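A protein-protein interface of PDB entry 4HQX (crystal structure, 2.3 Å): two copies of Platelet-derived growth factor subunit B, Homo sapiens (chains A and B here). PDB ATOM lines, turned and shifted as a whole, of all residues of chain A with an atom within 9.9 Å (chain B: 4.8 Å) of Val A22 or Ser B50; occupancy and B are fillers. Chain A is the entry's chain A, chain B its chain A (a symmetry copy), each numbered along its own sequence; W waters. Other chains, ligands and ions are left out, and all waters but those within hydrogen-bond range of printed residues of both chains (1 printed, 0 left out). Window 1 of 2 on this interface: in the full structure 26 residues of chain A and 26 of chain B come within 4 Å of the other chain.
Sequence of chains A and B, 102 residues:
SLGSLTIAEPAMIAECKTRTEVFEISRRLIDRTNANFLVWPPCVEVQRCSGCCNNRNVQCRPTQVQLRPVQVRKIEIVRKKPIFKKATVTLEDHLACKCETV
The side-chain carboxylate (OE2) of Glu A45 lies within salt-bridge range of the side-chain amino group (NZ) of Lys B17 (3.9 Å).
The side-chain sulfur (SG) of Cys B52 forms a disulfide with the side-chain sulfur (SG) of Cys A43.
OE2 of Glu A45 is in salt-bridge range of NE of Arg B19 (3.0 Å).
N of Ala B14 lies within hydrogen-bond range of O of Cys A43 (2.8 Å).
N of Phe A23 sits at hydrogen-bond distance from O of Val A44, 2.8 Å away.
The backbone carbonyl oxygen of Ala B14 is in hydrogen-bond range of the backbone NH of Cys B52 (3.0 Å).
NH1 of Arg B19 sits at hydrogen-bond distance from O of Ser B50 (2.8 Å).
N of Arg B48 lies within hydrogen-bond range of O of Arg B19, at 2.8 Å.
The backbone carbonyl oxygen (O) of Glu B15 lies within hydrogen-bond range of the guanidinium group (NH2) of Arg B19, at 2.8 Å.
O of Lys B17 is in hydrogen-bond range of N of Ser B50, at 2.8 Å.
Ala B14 touches Val A22.
CG2 of Val A22 touches NH1 of Arg B19, at 3.8 Å.
OG of Ser B50 touches CG2 of Val A22, 3.9 Å away.
CG2 of Val A22 touches N of Gly B51, 3.8 Å away.
C of Val A44 touches CB of Ala B14 (3.8 Å).
CB of Ala B14 touches N of Glu A45, at 3.97 Å.
Of the printed residues of chain B, Val A22 touches Ala B14, Arg B19, Ser B50 and Gly B51.
No residue of chain A comes within 4 Å of Cys B16.
Arg B19 touches just these residues of chain A: Val A22 and Glu A45.
Cys B49 touches none of the printed residues of chain A.
Printed residues of chain A within 4 Å of Cys B52: Cys A43 (2.2 Å).
Of the printed residues of chain B, Cys A43 touches Ala B14 and Cys B52.
Of the printed residues of chain B, Val A44 touches Ala B14.
Val A46 touches none of the printed residues of chain B.
The nearest residue of chain A that does not touch Ser B50 is Thr A20 (6.2 Å).
Of the 19 printed residues of chain A, 4 touch a printed residue of chain B.
Hydrophobic or aromatic side chains of chain A within 4 Å of the printed part of chain B: Val A22.
Of the 12 printed residues of chain B, 6 touch a printed residue of chain A.
Printed residues of chain B that touch a printed residue of chain A: Ala B14, Lys B17, Arg B19, Ser B50, Gly B51 and Cys B52.
Among the printed residues, 10 pairs touch across the chains.
Among the printed residues, Asp or Glu carboxylates within 4 Å of a Lys or Arg side-chain nitrogen of the other chain: Glu A45 with Lys B17 and Glu A45 with Arg B19.
3 positions are printed for both chains.
Of the 10 pairs that touch across the chains among the printed residues, none has its exchanged pair printed and touching as well.
Water W1 lies within hydrogen-bond range of the side-chain carboxylate (OE2) of Glu A45 (3.1 Å), the guanidinium group (NH2) of Arg B19 (3.2 Å) and the backbone NH (N) of Glu B15 (3.3 Å).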
ATOM      1  N   ARG A  19      -4.220 -23.935   4.062  1.00  0.00           N
ATOM      2  CA  ARG A  19      -3.867 -25.234   3.513  1.00  0.00           C
ATOM      3  C   ARG A  19      -3.161 -25.000   2.164  1.00  0.00           C
ATOM      4  O   ARG A  19      -3.303 -23.930   1.542  1.00  0.00           O
ATOM      5  CB  ARG A  19      -5.119 -26.098   3.311  1.00  0.00           C
ATOM      6  CG  ARG A  19      -5.772 -26.607   4.588  1.00  0.00           C
ATOM      7  CD  ARG A  19      -7.126 -27.266   4.339  1.00  0.00           C
ATOM      8  NE  ARG A  19      -7.774 -27.616   5.607  1.00  0.00           N
ATOM      9  CZ  ARG A  19      -8.599 -26.812   6.279  1.00  0.00           C
ATOM     10  NH1 ARG A  19      -8.922 -25.607   5.794  1.00  0.00           N
ATOM     11  NH2 ARG A  19      -9.120 -27.217   7.431  1.00  0.00           N
ATOM     12  N   THR A  20      -2.412 -26.003   1.724  1.00  0.00           N
ATOM     13  CA  THR A  20      -1.689 -25.954   0.463  1.00  0.00           C
ATOM     14  C   THR A  20      -2.643 -26.149  -0.722  1.00  0.00           C
ATOM     15  O   THR A  20      -3.334 -27.160  -0.799  1.00  0.00           O
ATOM     16  CB  THR A  20      -0.595 -27.041   0.444  1.00  0.00           C
ATOM     17  OG1 THR A  20       0.267 -26.866   1.581  1.00  0.00           O
ATOM     18  CG2 THR A  20       0.238 -26.959  -0.831  1.00  0.00           C
ATOM     19  N   GLU A  21      -2.681 -25.185  -1.640  1.00  0.00           N
ATOM     20  CA  GLU A  21      -3.484 -25.318  -2.858  1.00  0.00           C
ATOM     21  C   GLU A  21      -2.658 -25.221  -4.157  1.00  0.00           C
ATOM     22  O   GLU A  21      -1.545 -24.707  -4.155  1.00  0.00           O
ATOM     23  CB  GLU A  21      -4.636 -24.313  -2.852  1.00  0.00           C
ATOM     24  CG  GLU A  21      -5.886 -24.852  -2.165  1.00  0.00           C
ATOM     25  CD  GLU A  21      -6.941 -23.790  -1.926  1.00  0.00           C
ATOM     26  OE1 GLU A  21      -6.976 -22.800  -2.680  1.00  0.00           O
ATOM     27  OE2 GLU A  21      -7.742 -23.937  -0.976  1.00  0.00           O
ATOM     28  N   VAL A  22      -3.194 -25.735  -5.261  1.00  0.00           N
ATOM     29  CA  VAL A  22      -2.472 -25.655  -6.527  1.00  0.00           C
ATOM     30  C   VAL A  22      -2.845 -24.357  -7.242  1.00  0.00           C
ATOM     31  O   VAL A  22      -4.015 -24.062  -7.436  1.00  0.00           O
ATOM     32  CB  VAL A  22      -2.701 -26.885  -7.427  1.00  0.00           C
ATOM     33  CG1 VAL A  22      -1.978 -26.720  -8.763  1.00  0.00           C
ATOM     34  CG2 VAL A  22      -2.208 -28.145  -6.729  1.00  0.00           C
ATOM     35  N   PHE A  23      -1.829 -23.570  -7.576  1.00  0.00           N
ATOM     36  CA  PHE A  23      -1.994 -22.327  -8.306  1.00  0.00           C
ATOM     37  C   PHE A  23      -1.465 -22.518  -9.731  1.00  0.00           C
ATOM     38  O   PHE A  23      -0.330 -22.944  -9.938  1.00  0.00           O
ATOM     39  CB  PHE A  23      -1.247 -21.196  -7.580  1.00  0.00           C
ATOM     40  CG  PHE A  23      -1.370 -19.838  -8.242  1.00  0.00           C
ATOM     41  CD1 PHE A  23      -0.291 -19.289  -8.949  1.00  0.00           C
ATOM     42  CD2 PHE A  23      -2.550 -19.095  -8.148  1.00  0.00           C
ATOM     43  CE1 PHE A  23      -0.401 -18.035  -9.554  1.00  0.00           C
ATOM     44  CE2 PHE A  23      -2.659 -17.841  -8.755  1.00  0.00           C
ATOM     45  CZ  PHE A  23      -1.583 -17.315  -9.460  1.00  0.00           C
ATOM     46  N   GLU A  24      -2.303 -22.222 -10.714  1.00  0.00           N
ATOM     47  CA  GLU A  24      -1.876 -22.272 -12.091  1.00  0.00           C
ATOM     48  C   GLU A  24      -1.228 -20.927 -12.434  1.00  0.00           C
ATOM     49  O   GLU A  24      -1.779 -19.866 -12.135  1.00  0.00           O
ATOM     50  CB  GLU A  24      -3.060 -22.565 -13.001  1.00  0.00           C
ATOM     51  CG  GLU A  24      -2.662 -23.084 -14.372  1.00  0.00           C
ATOM     52  CD  GLU A  24      -3.861 -23.502 -15.213  1.00  0.00           C
ATOM     53  OE1 GLU A  24      -4.989 -23.558 -14.669  1.00  0.00           O
ATOM     54  OE2 GLU A  24      -3.675 -23.778 -16.418  1.00  0.00           O
ATOM     55  N   ILE A  25      -0.033 -20.980 -13.016  1.00  0.00           N
ATOM     56  CA  ILE A  25       0.670 -19.773 -13.416  1.00  0.00           C
ATOM     57  C   ILE A  25       0.027 -19.256 -14.689  1.00  0.00           C
ATOM     58  O   ILE A  25      -0.132 -19.992 -15.651  1.00  0.00           O
ATOM     59  CB  ILE A  25       2.183 -20.020 -13.571  1.00  0.00           C
ATOM     60  CG1 ILE A  25       2.852 -19.894 -12.201  1.00  0.00           C
ATOM     61  CG2 ILE A  25       2.810 -19.025 -14.545  1.00  0.00           C
ATOM     62  CD1 ILE A  25       3.976 -20.873 -11.990  1.00  0.00           C
ATOM     63  N   PRO A  41       7.564 -23.890 -14.614  1.00  0.00           N
ATOM     64  CA  PRO A  41       6.455 -24.870 -14.578  1.00  0.00           C
ATOM     65  C   PRO A  41       5.069 -24.215 -14.776  1.00  0.00           C
ATOM     66  O   PRO A  41       4.954 -22.991 -14.635  1.00  0.00           O
ATOM     67  CB  PRO A  41       6.568 -25.456 -13.172  1.00  0.00           C
ATOM     68  CG  PRO A  41       7.121 -24.334 -12.354  1.00  0.00           C
ATOM     69  CD  PRO A  41       8.003 -23.508 -13.258  1.00  0.00           C
ATOM     70  N   PRO A  42       4.029 -25.018 -15.103  1.00  0.00           N
ATOM     71  CA  PRO A  42       2.681 -24.468 -15.269  1.00  0.00           C
ATOM     72  C   PRO A  42       1.912 -24.217 -13.953  1.00  0.00           C
ATOM     73  O   PRO A  42       0.963 -23.412 -13.947  1.00  0.00           O
ATOM     74  CB  PRO A  42       1.966 -25.528 -16.114  1.00  0.00           C
ATOM     75  CG  PRO A  42       2.686 -26.805 -15.821  1.00  0.00           C
ATOM     76  CD  PRO A  42       4.064 -26.480 -15.305  1.00  0.00           C
ATOM     77  N   CYS A  43       2.313 -24.877 -12.858  1.00  0.00           N
ATOM     78  CA  CYS A  43       1.607 -24.770 -11.577  1.00  0.00           C
ATOM     79  C   CYS A  43       2.542 -24.849 -10.388  1.00  0.00           C
ATOM     80  O   CYS A  43       3.516 -25.600 -10.411  1.00  0.00           O
ATOM     81  CB  CYS A  43       0.602 -25.902 -11.425  1.00  0.00           C
ATOM     82  SG  CYS A  43      -0.549 -26.050 -12.792  1.00  0.00           S
ATOM     83  N   VAL A  44       2.213 -24.103  -9.337  1.00  0.00           N
ATOM     84  CA  VAL A  44       2.993 -24.112  -8.100  1.00  0.00           C
ATOM     85  C   VAL A  44       2.076 -24.190  -6.877  1.00  0.00           C
ATOM     86  O   VAL A  44       0.893 -23.848  -6.950  1.00  0.00           O
ATOM     87  CB  VAL A  44       3.890 -22.863  -7.974  1.00  0.00           C
ATOM     88  CG1 VAL A  44       4.907 -22.815  -9.110  1.00  0.00           C
ATOM     89  CG2 VAL A  44       3.042 -21.602  -7.968  1.00  0.00           C
ATOM     90  N   GLU A  45       2.639 -24.647  -5.764  1.00  0.00           N
ATOM     91  CA  GLU A  45       1.933 -24.692  -4.501  1.00  0.00           C
ATOM     92  C   GLU A  45       1.864 -23.312  -3.890  1.00  0.00           C
ATOM     93  O   GLU A  45       2.832 -22.553  -3.924  1.00  0.00           O
ATOM     94  CB  GLU A  45       2.606 -25.680  -3.541  1.00  0.00           C
ATOM     95  CG  GLU A  45       2.286 -27.124  -3.900  1.00  0.00           C
ATOM     96  CD  GLU A  45       2.832 -28.153  -2.924  1.00  0.00           C
ATOM     97  OE1 GLU A  45       3.619 -27.786  -2.021  1.00  0.00           O
ATOM     98  OE2 GLU A  45       2.473 -29.349  -3.069  1.00  0.00           O
ATOM     99  N   VAL A  46       0.695 -22.973  -3.368  1.00  0.00           N
ATOM    100  CA  VAL A  46       0.536 -21.772  -2.566  1.00  0.00           C
ATOM    101  C   VAL A  46      -0.257 -22.147  -1.314  1.00  0.00           C
ATOM    102  O   VAL A  46      -0.873 -23.224  -1.250  1.00  0.00           O
ATOM    103  CB  VAL A  46      -0.190 -20.653  -3.328  1.00  0.00           C
ATOM    104  CG1 VAL A  46       0.658 -20.160  -4.497  1.00  0.00           C
ATOM    105  CG2 VAL A  46      -1.558 -21.123  -3.805  1.00  0.00           C
ATOM    106  N   GLN A  47      -0.226 -21.266  -0.319  1.00  0.00           N
ATOM    107  CA  GLN A  47      -1.016 -21.434   0.894  1.00  0.00           C
ATOM    108  C   GLN A  47      -2.272 -20.579   0.765  1.00  0.00           C
ATOM    109  O   GLN A  47      -2.192 -19.398   0.409  1.00  0.00           O
ATOM    110  CB  GLN A  47      -0.209 -21.023   2.129  1.00  0.00           C
ATOM    111  CG  GLN A  47       1.016 -21.877   2.366  1.00  0.00           C
ATOM    112  CD  GLN A  47       0.651 -23.296   2.726  1.00  0.00           C
ATOM    113  OE1 GLN A  47       0.017 -23.537   3.755  1.00  0.00           O
ATOM    114  NE2 GLN A  47       1.045 -24.251   1.883  1.00  0.00           N
ATOM    115  N   ARG A  48      -3.425 -21.194   1.036  1.00  0.00           N
ATOM    116  CA  ARG A  48      -4.711 -20.518   0.935  1.00  0.00           C
ATOM    117  C   ARG A  48      -5.613 -20.802   2.145  1.00  0.00           C
ATOM    118  O   ARG A  48      -5.602 -21.917   2.710  1.00  0.00           O
ATOM    119  CB  ARG A  48      -5.425 -20.897  -0.378  1.00  0.00           C
ATOM    120  CG  ARG A  48      -4.763 -20.367  -1.652  1.00  0.00           C
ATOM    121  CD  ARG A  48      -4.952 -18.859  -1.813  1.00  0.00           C
ATOM    122  NE  ARG A  48      -3.824 -18.215  -2.497  1.00  0.00           N
ATOM    123  CZ  ARG A  48      -3.848 -17.831  -3.768  1.00  0.00           C
ATOM    124  NH1 ARG A  48      -4.933 -18.022  -4.508  1.00  0.00           N
ATOM    125  NH2 ARG A  48      -2.793 -17.253  -4.312  1.00  0.00           N
ATOM    126  N   ARG A  68       5.292 -13.447  -2.635  1.00  0.00           N
ATOM    127  CA  ARG A  68       6.430 -14.340  -2.829  1.00  0.00           C
ATOM    128  C   ARG A  68       6.765 -14.398  -4.318  1.00  0.00           C
ATOM    129  O   ARG A  68       5.987 -14.916  -5.124  1.00  0.00           O
ATOM    130  CB  ARG A  68       6.125 -15.726  -2.265  1.00  0.00           C
ATOM    131  CG  ARG A  68       7.257 -16.730  -2.406  1.00  0.00           C
ATOM    132  CD  ARG A  68       7.017 -17.986  -1.574  1.00  0.00           C
ATOM    133  NE  ARG A  68       5.676 -18.539  -1.780  1.00  0.00           N
ATOM    134  CZ  ARG A  68       5.385 -19.582  -2.559  1.00  0.00           C
ATOM    135  NH1 ARG A  68       6.337 -20.221  -3.232  1.00  0.00           N
ATOM    136  NH2 ARG A  68       4.126 -19.992  -2.665  1.00  0.00           N
ATOM    137  N   LEU A  91       3.816 -14.631  -6.442  1.00  0.00           N
ATOM    138  CA  LEU A  91       2.787 -15.434  -5.790  1.00  0.00           C
ATOM    139  C   LEU A  91       2.239 -14.758  -4.531  1.00  0.00           C
ATOM    140  O   LEU A  91       2.959 -14.019  -3.849  1.00  0.00           O
ATOM    141  CB  LEU A  91       3.353 -16.796  -5.406  1.00  0.00           C
ATOM    142  CG  LEU A  91       3.939 -17.683  -6.502  1.00  0.00           C
ATOM    143  CD1 LEU A  91       4.392 -18.996  -5.889  1.00  0.00           C
ATOM    144  CD2 LEU A  91       2.954 -17.928  -7.643  1.00  0.00           C
ATOM    145  N   GLU A  92       0.969 -15.025  -4.221  1.00  0.00           N
ATOM    146  CA  GLU A  92       0.389 -14.621  -2.941  1.00  0.00           C
ATOM    147  C   GLU A  92       0.043 -15.816  -2.048  1.00  0.00           C
ATOM    148  O   GLU A  92      -0.814 -16.632  -2.378  1.00  0.00           O
ATOM    149  CB  GLU A  92      -0.827 -13.733  -3.152  1.00  0.00           C
ATOM    150  CG  GLU A  92      -1.370 -13.168  -1.860  1.00  0.00           C
ATOM    151  CD  GLU A  92      -2.574 -12.285  -2.082  1.00  0.00           C
ATOM    152  OE1 GLU A  92      -2.378 -11.087  -2.372  1.00  0.00           O
ATOM    153  OE2 GLU A  92      -3.713 -12.791  -1.961  1.00  0.00           O
ATOM    154  N   ASP A  93       0.745 -15.920  -0.923  1.00  0.00           N
ATOM    155  CA  ASP A  93       0.419 -16.879   0.127  1.00  0.00           C
ATOM    156  C   ASP A  93      -0.507 -16.240   1.157  1.00  0.00           C
ATOM    157  O   ASP A  93      -0.343 -15.057   1.498  1.00  0.00           O
ATOM    158  CB  ASP A  93       1.683 -17.343   0.842  1.00  0.00           C
ATOM    159  CG  ASP A  93       2.441 -18.389   0.076  1.00  0.00           C
ATOM    160  OD1 ASP A  93       1.844 -19.086  -0.753  1.00  0.00           O
ATOM    161  OD2 ASP A  93       3.646 -18.532   0.320  1.00  0.00           O
ATOM    162  N   ALA B  14       3.922 -27.946  -8.913  1.00  0.00           N
ATOM    163  CA  ALA B  14       2.947 -28.624  -8.071  1.00  0.00           C
ATOM    164  C   ALA B  14       2.683 -29.950  -8.760  1.00  0.00           C
ATOM    165  O   ALA B  14       1.907 -30.027  -9.720  1.00  0.00           O
ATOM    166  CB  ALA B  14       1.668 -27.811  -7.953  1.00  0.00           C
ATOM    167  N   GLU B  15       3.368 -30.990  -8.301  1.00  0.00           N
ATOM    168  CA  GLU B  15       3.240 -32.294  -8.933  1.00  0.00           C
ATOM    169  C   GLU B  15       1.899 -32.943  -8.612  1.00  0.00           C
ATOM    170  O   GLU B  15       1.187 -32.524  -7.680  1.00  0.00           O
ATOM    171  CB  GLU B  15       4.398 -33.213  -8.549  1.00  0.00           C
ATOM    172  CG  GLU B  15       4.715 -33.220  -7.072  1.00  0.00           C
ATOM    173  CD  GLU B  15       5.871 -34.136  -6.752  1.00  0.00           C
ATOM    174  OE1 GLU B  15       6.756 -34.317  -7.628  1.00  0.00           O
ATOM    175  OE2 GLU B  15       5.893 -34.670  -5.621  1.00  0.00           O
ATOM    176  N   CYS B  16       1.566 -33.945  -9.420  1.00  0.00           N
ATOM    177  CA  CYS B  16       0.347 -34.703  -9.293  1.00  0.00           C
ATOM    178  C   CYS B  16       0.499 -35.627  -8.111  1.00  0.00           C
ATOM    179  O   CYS B  16       1.346 -36.518  -8.126  1.00  0.00           O
ATOM    180  CB  CYS B  16       0.113 -35.504 -10.558  1.00  0.00           C
ATOM    181  SG  CYS B  16      -1.243 -36.673 -10.431  1.00  0.00           S
ATOM    182  N   LYS B  17      -0.294 -35.378  -7.071  1.00  0.00           N
ATOM    183  CA  LYS B  17      -0.254 -36.169  -5.843  1.00  0.00           C
ATOM    184  C   LYS B  17      -1.446 -35.851  -4.932  1.00  0.00           C
ATOM    185  O   LYS B  17      -2.277 -34.986  -5.256  1.00  0.00           O
ATOM    186  CB  LYS B  17       1.049 -35.926  -5.099  1.00  0.00           C
ATOM    187  CG  LYS B  17       1.241 -34.504  -4.635  1.00  0.00           C
ATOM    188  CD  LYS B  17       2.369 -34.431  -3.638  1.00  0.00           C
ATOM    189  CE  LYS B  17       2.467 -33.043  -3.058  1.00  0.00           C
ATOM    190  NZ  LYS B  17       3.703 -32.911  -2.240  1.00  0.00           N
ATOM    191  N   ARG B  19      -3.281 -34.243  -1.766  1.00  0.00           N
ATOM    192  CA  ARG B  19      -3.236 -33.116  -0.850  1.00  0.00           C
ATOM    193  C   ARG B  19      -4.569 -33.080  -0.079  1.00  0.00           C
ATOM    194  O   ARG B  19      -5.582 -33.654  -0.521  1.00  0.00           O
ATOM    195  CB  ARG B  19      -3.033 -31.801  -1.614  1.00  0.00           C
ATOM    196  CG  ARG B  19      -1.650 -31.606  -2.219  1.00  0.00           C
ATOM    197  CD  ARG B  19      -1.574 -30.396  -3.148  1.00  0.00           C
ATOM    198  NE  ARG B  19      -0.266 -30.331  -3.808  1.00  0.00           N
ATOM    199  CZ  ARG B  19       0.016 -30.901  -4.980  1.00  0.00           C
ATOM    200  NH1 ARG B  19      -0.927 -31.561  -5.662  1.00  0.00           N
ATOM    201  NH2 ARG B  19       1.240 -30.798  -5.485  1.00  0.00           N
ATOM    202  N   GLU B  21      -7.944 -31.650   1.057  1.00  0.00           N
ATOM    203  CA  GLU B  21      -8.978 -30.727   0.583  1.00  0.00           C
ATOM    204  C   GLU B  21     -10.211 -30.650   1.508  1.00  0.00           C
ATOM    205  O   GLU B  21     -10.444 -31.542   2.316  1.00  0.00           O
ATOM    206  CB  GLU B  21      -9.379 -31.065  -0.854  1.00  0.00           C
ATOM    207  CG  GLU B  21      -8.509 -30.363  -1.889  1.00  0.00           C
ATOM    208  CD  GLU B  21      -8.723 -30.879  -3.300  1.00  0.00           C
ATOM    209  OE1 GLU B  21      -9.824 -31.381  -3.592  1.00  0.00           O
ATOM    210  OE2 GLU B  21      -7.787 -30.791  -4.124  1.00  0.00           O
ATOM    211  N   ARG B  48      -7.195 -35.644  -1.613  1.00  0.00           N
ATOM    212  CA  ARG B  48      -7.552 -35.614  -3.026  1.00  0.00           C
ATOM    213  C   ARG B  48      -6.320 -35.471  -3.932  1.00  0.00           C
ATOM    214  O   ARG B  48      -5.337 -34.784  -3.582  1.00  0.00           O
ATOM    215  CB  ARG B  48      -8.569 -34.490  -3.308  1.00  0.00           C
ATOM    216  CG  ARG B  48      -9.958 -34.708  -2.705  1.00  0.00           C
ATOM    217  CD  ARG B  48     -10.738 -35.799  -3.436  1.00  0.00           C
ATOM    218  NE  ARG B  48     -11.649 -36.537  -2.552  1.00  0.00           N
ATOM    219  CZ  ARG B  48     -12.963 -36.345  -2.513  1.00  0.00           C
ATOM    220  NH1 ARG B  48     -13.535 -35.442  -3.300  1.00  0.00           N
ATOM    221  NH2 ARG B  48     -13.717 -37.053  -1.693  1.00  0.00           N
ATOM    222  N   CYS B  49      -6.372 -36.134  -5.086  1.00  0.00           N
ATOM    223  CA  CYS B  49      -5.357 -35.966  -6.120  1.00  0.00           C
ATOM    224  C   CYS B  49      -5.451 -34.549  -6.686  1.00  0.00           C
ATOM    225  O   CYS B  49      -6.524 -34.116  -7.095  1.00  0.00           O
ATOM    226  CB  CYS B  49      -5.550 -36.990  -7.244  1.00  0.00           C
ATOM    227  SG  CYS B  49      -5.091 -38.686  -6.805  1.00  0.00           S
ATOM    228  N   SER B  50      -4.341 -33.819  -6.677  1.00  0.00           N
ATOM    229  CA  SER B  50      -4.273 -32.537  -7.366  1.00  0.00           C
ATOM    230  C   SER B  50      -2.884 -32.313  -7.989  1.00  0.00           C
ATOM    231  O   SER B  50      -1.952 -33.092  -7.772  1.00  0.00           O
ATOM    232  CB  SER B  50      -4.636 -31.400  -6.413  1.00  0.00           C
ATOM    233  OG  SER B  50      -3.778 -31.408  -5.288  1.00  0.00           O
ATOM    234  N   GLY B  51      -2.753 -31.251  -8.767  1.00  0.00           N
ATOM    235  CA  GLY B  51      -1.464 -30.913  -9.337  1.00  0.00           C
ATOM    236  C   GLY B  51      -1.504 -31.002 -10.842  1.00  0.00           C
ATOM    237  O   GLY B  51      -2.545 -31.287 -11.434  1.00  0.00           O
ATOM    238  N   CYS B  52      -0.355 -30.765 -11.466  1.00  0.00           N
ATOM    239  CA  CYS B  52      -0.291 -30.641 -12.916  1.00  0.00           C
ATOM    240  C   CYS B  52       0.721 -31.568 -13.529  1.00  0.00           C
ATOM    241  O   CYS B  52       1.854 -31.650 -13.071  1.00  0.00           O
ATOM    242  CB  CYS B  52       0.016 -29.204 -13.297  1.00  0.00           C
ATOM    243  SG  CYS B  52      -1.231 -28.102 -12.607  1.00  0.00           S
ATOM    244  N   CYS B  60      -4.607 -35.489 -13.873  1.00  0.00           N
ATOM    245  CA  CYS B  60      -4.148 -36.087 -12.619  1.00  0.00           C
ATOM    246  C   CYS B  60      -5.276 -36.841 -11.900  1.00  0.00           C
ATOM    247  O   CYS B  60      -6.093 -36.221 -11.232  1.00  0.00           O
ATOM    248  CB  CYS B  60      -3.575 -34.998 -11.714  1.00  0.00           C
ATOM    249  SG  CYS B  60      -2.964 -35.612 -10.135  1.00  0.00           S
HETATM  250  O   HOH W   1       4.369 -30.328  -5.277  1.00  0.00           O
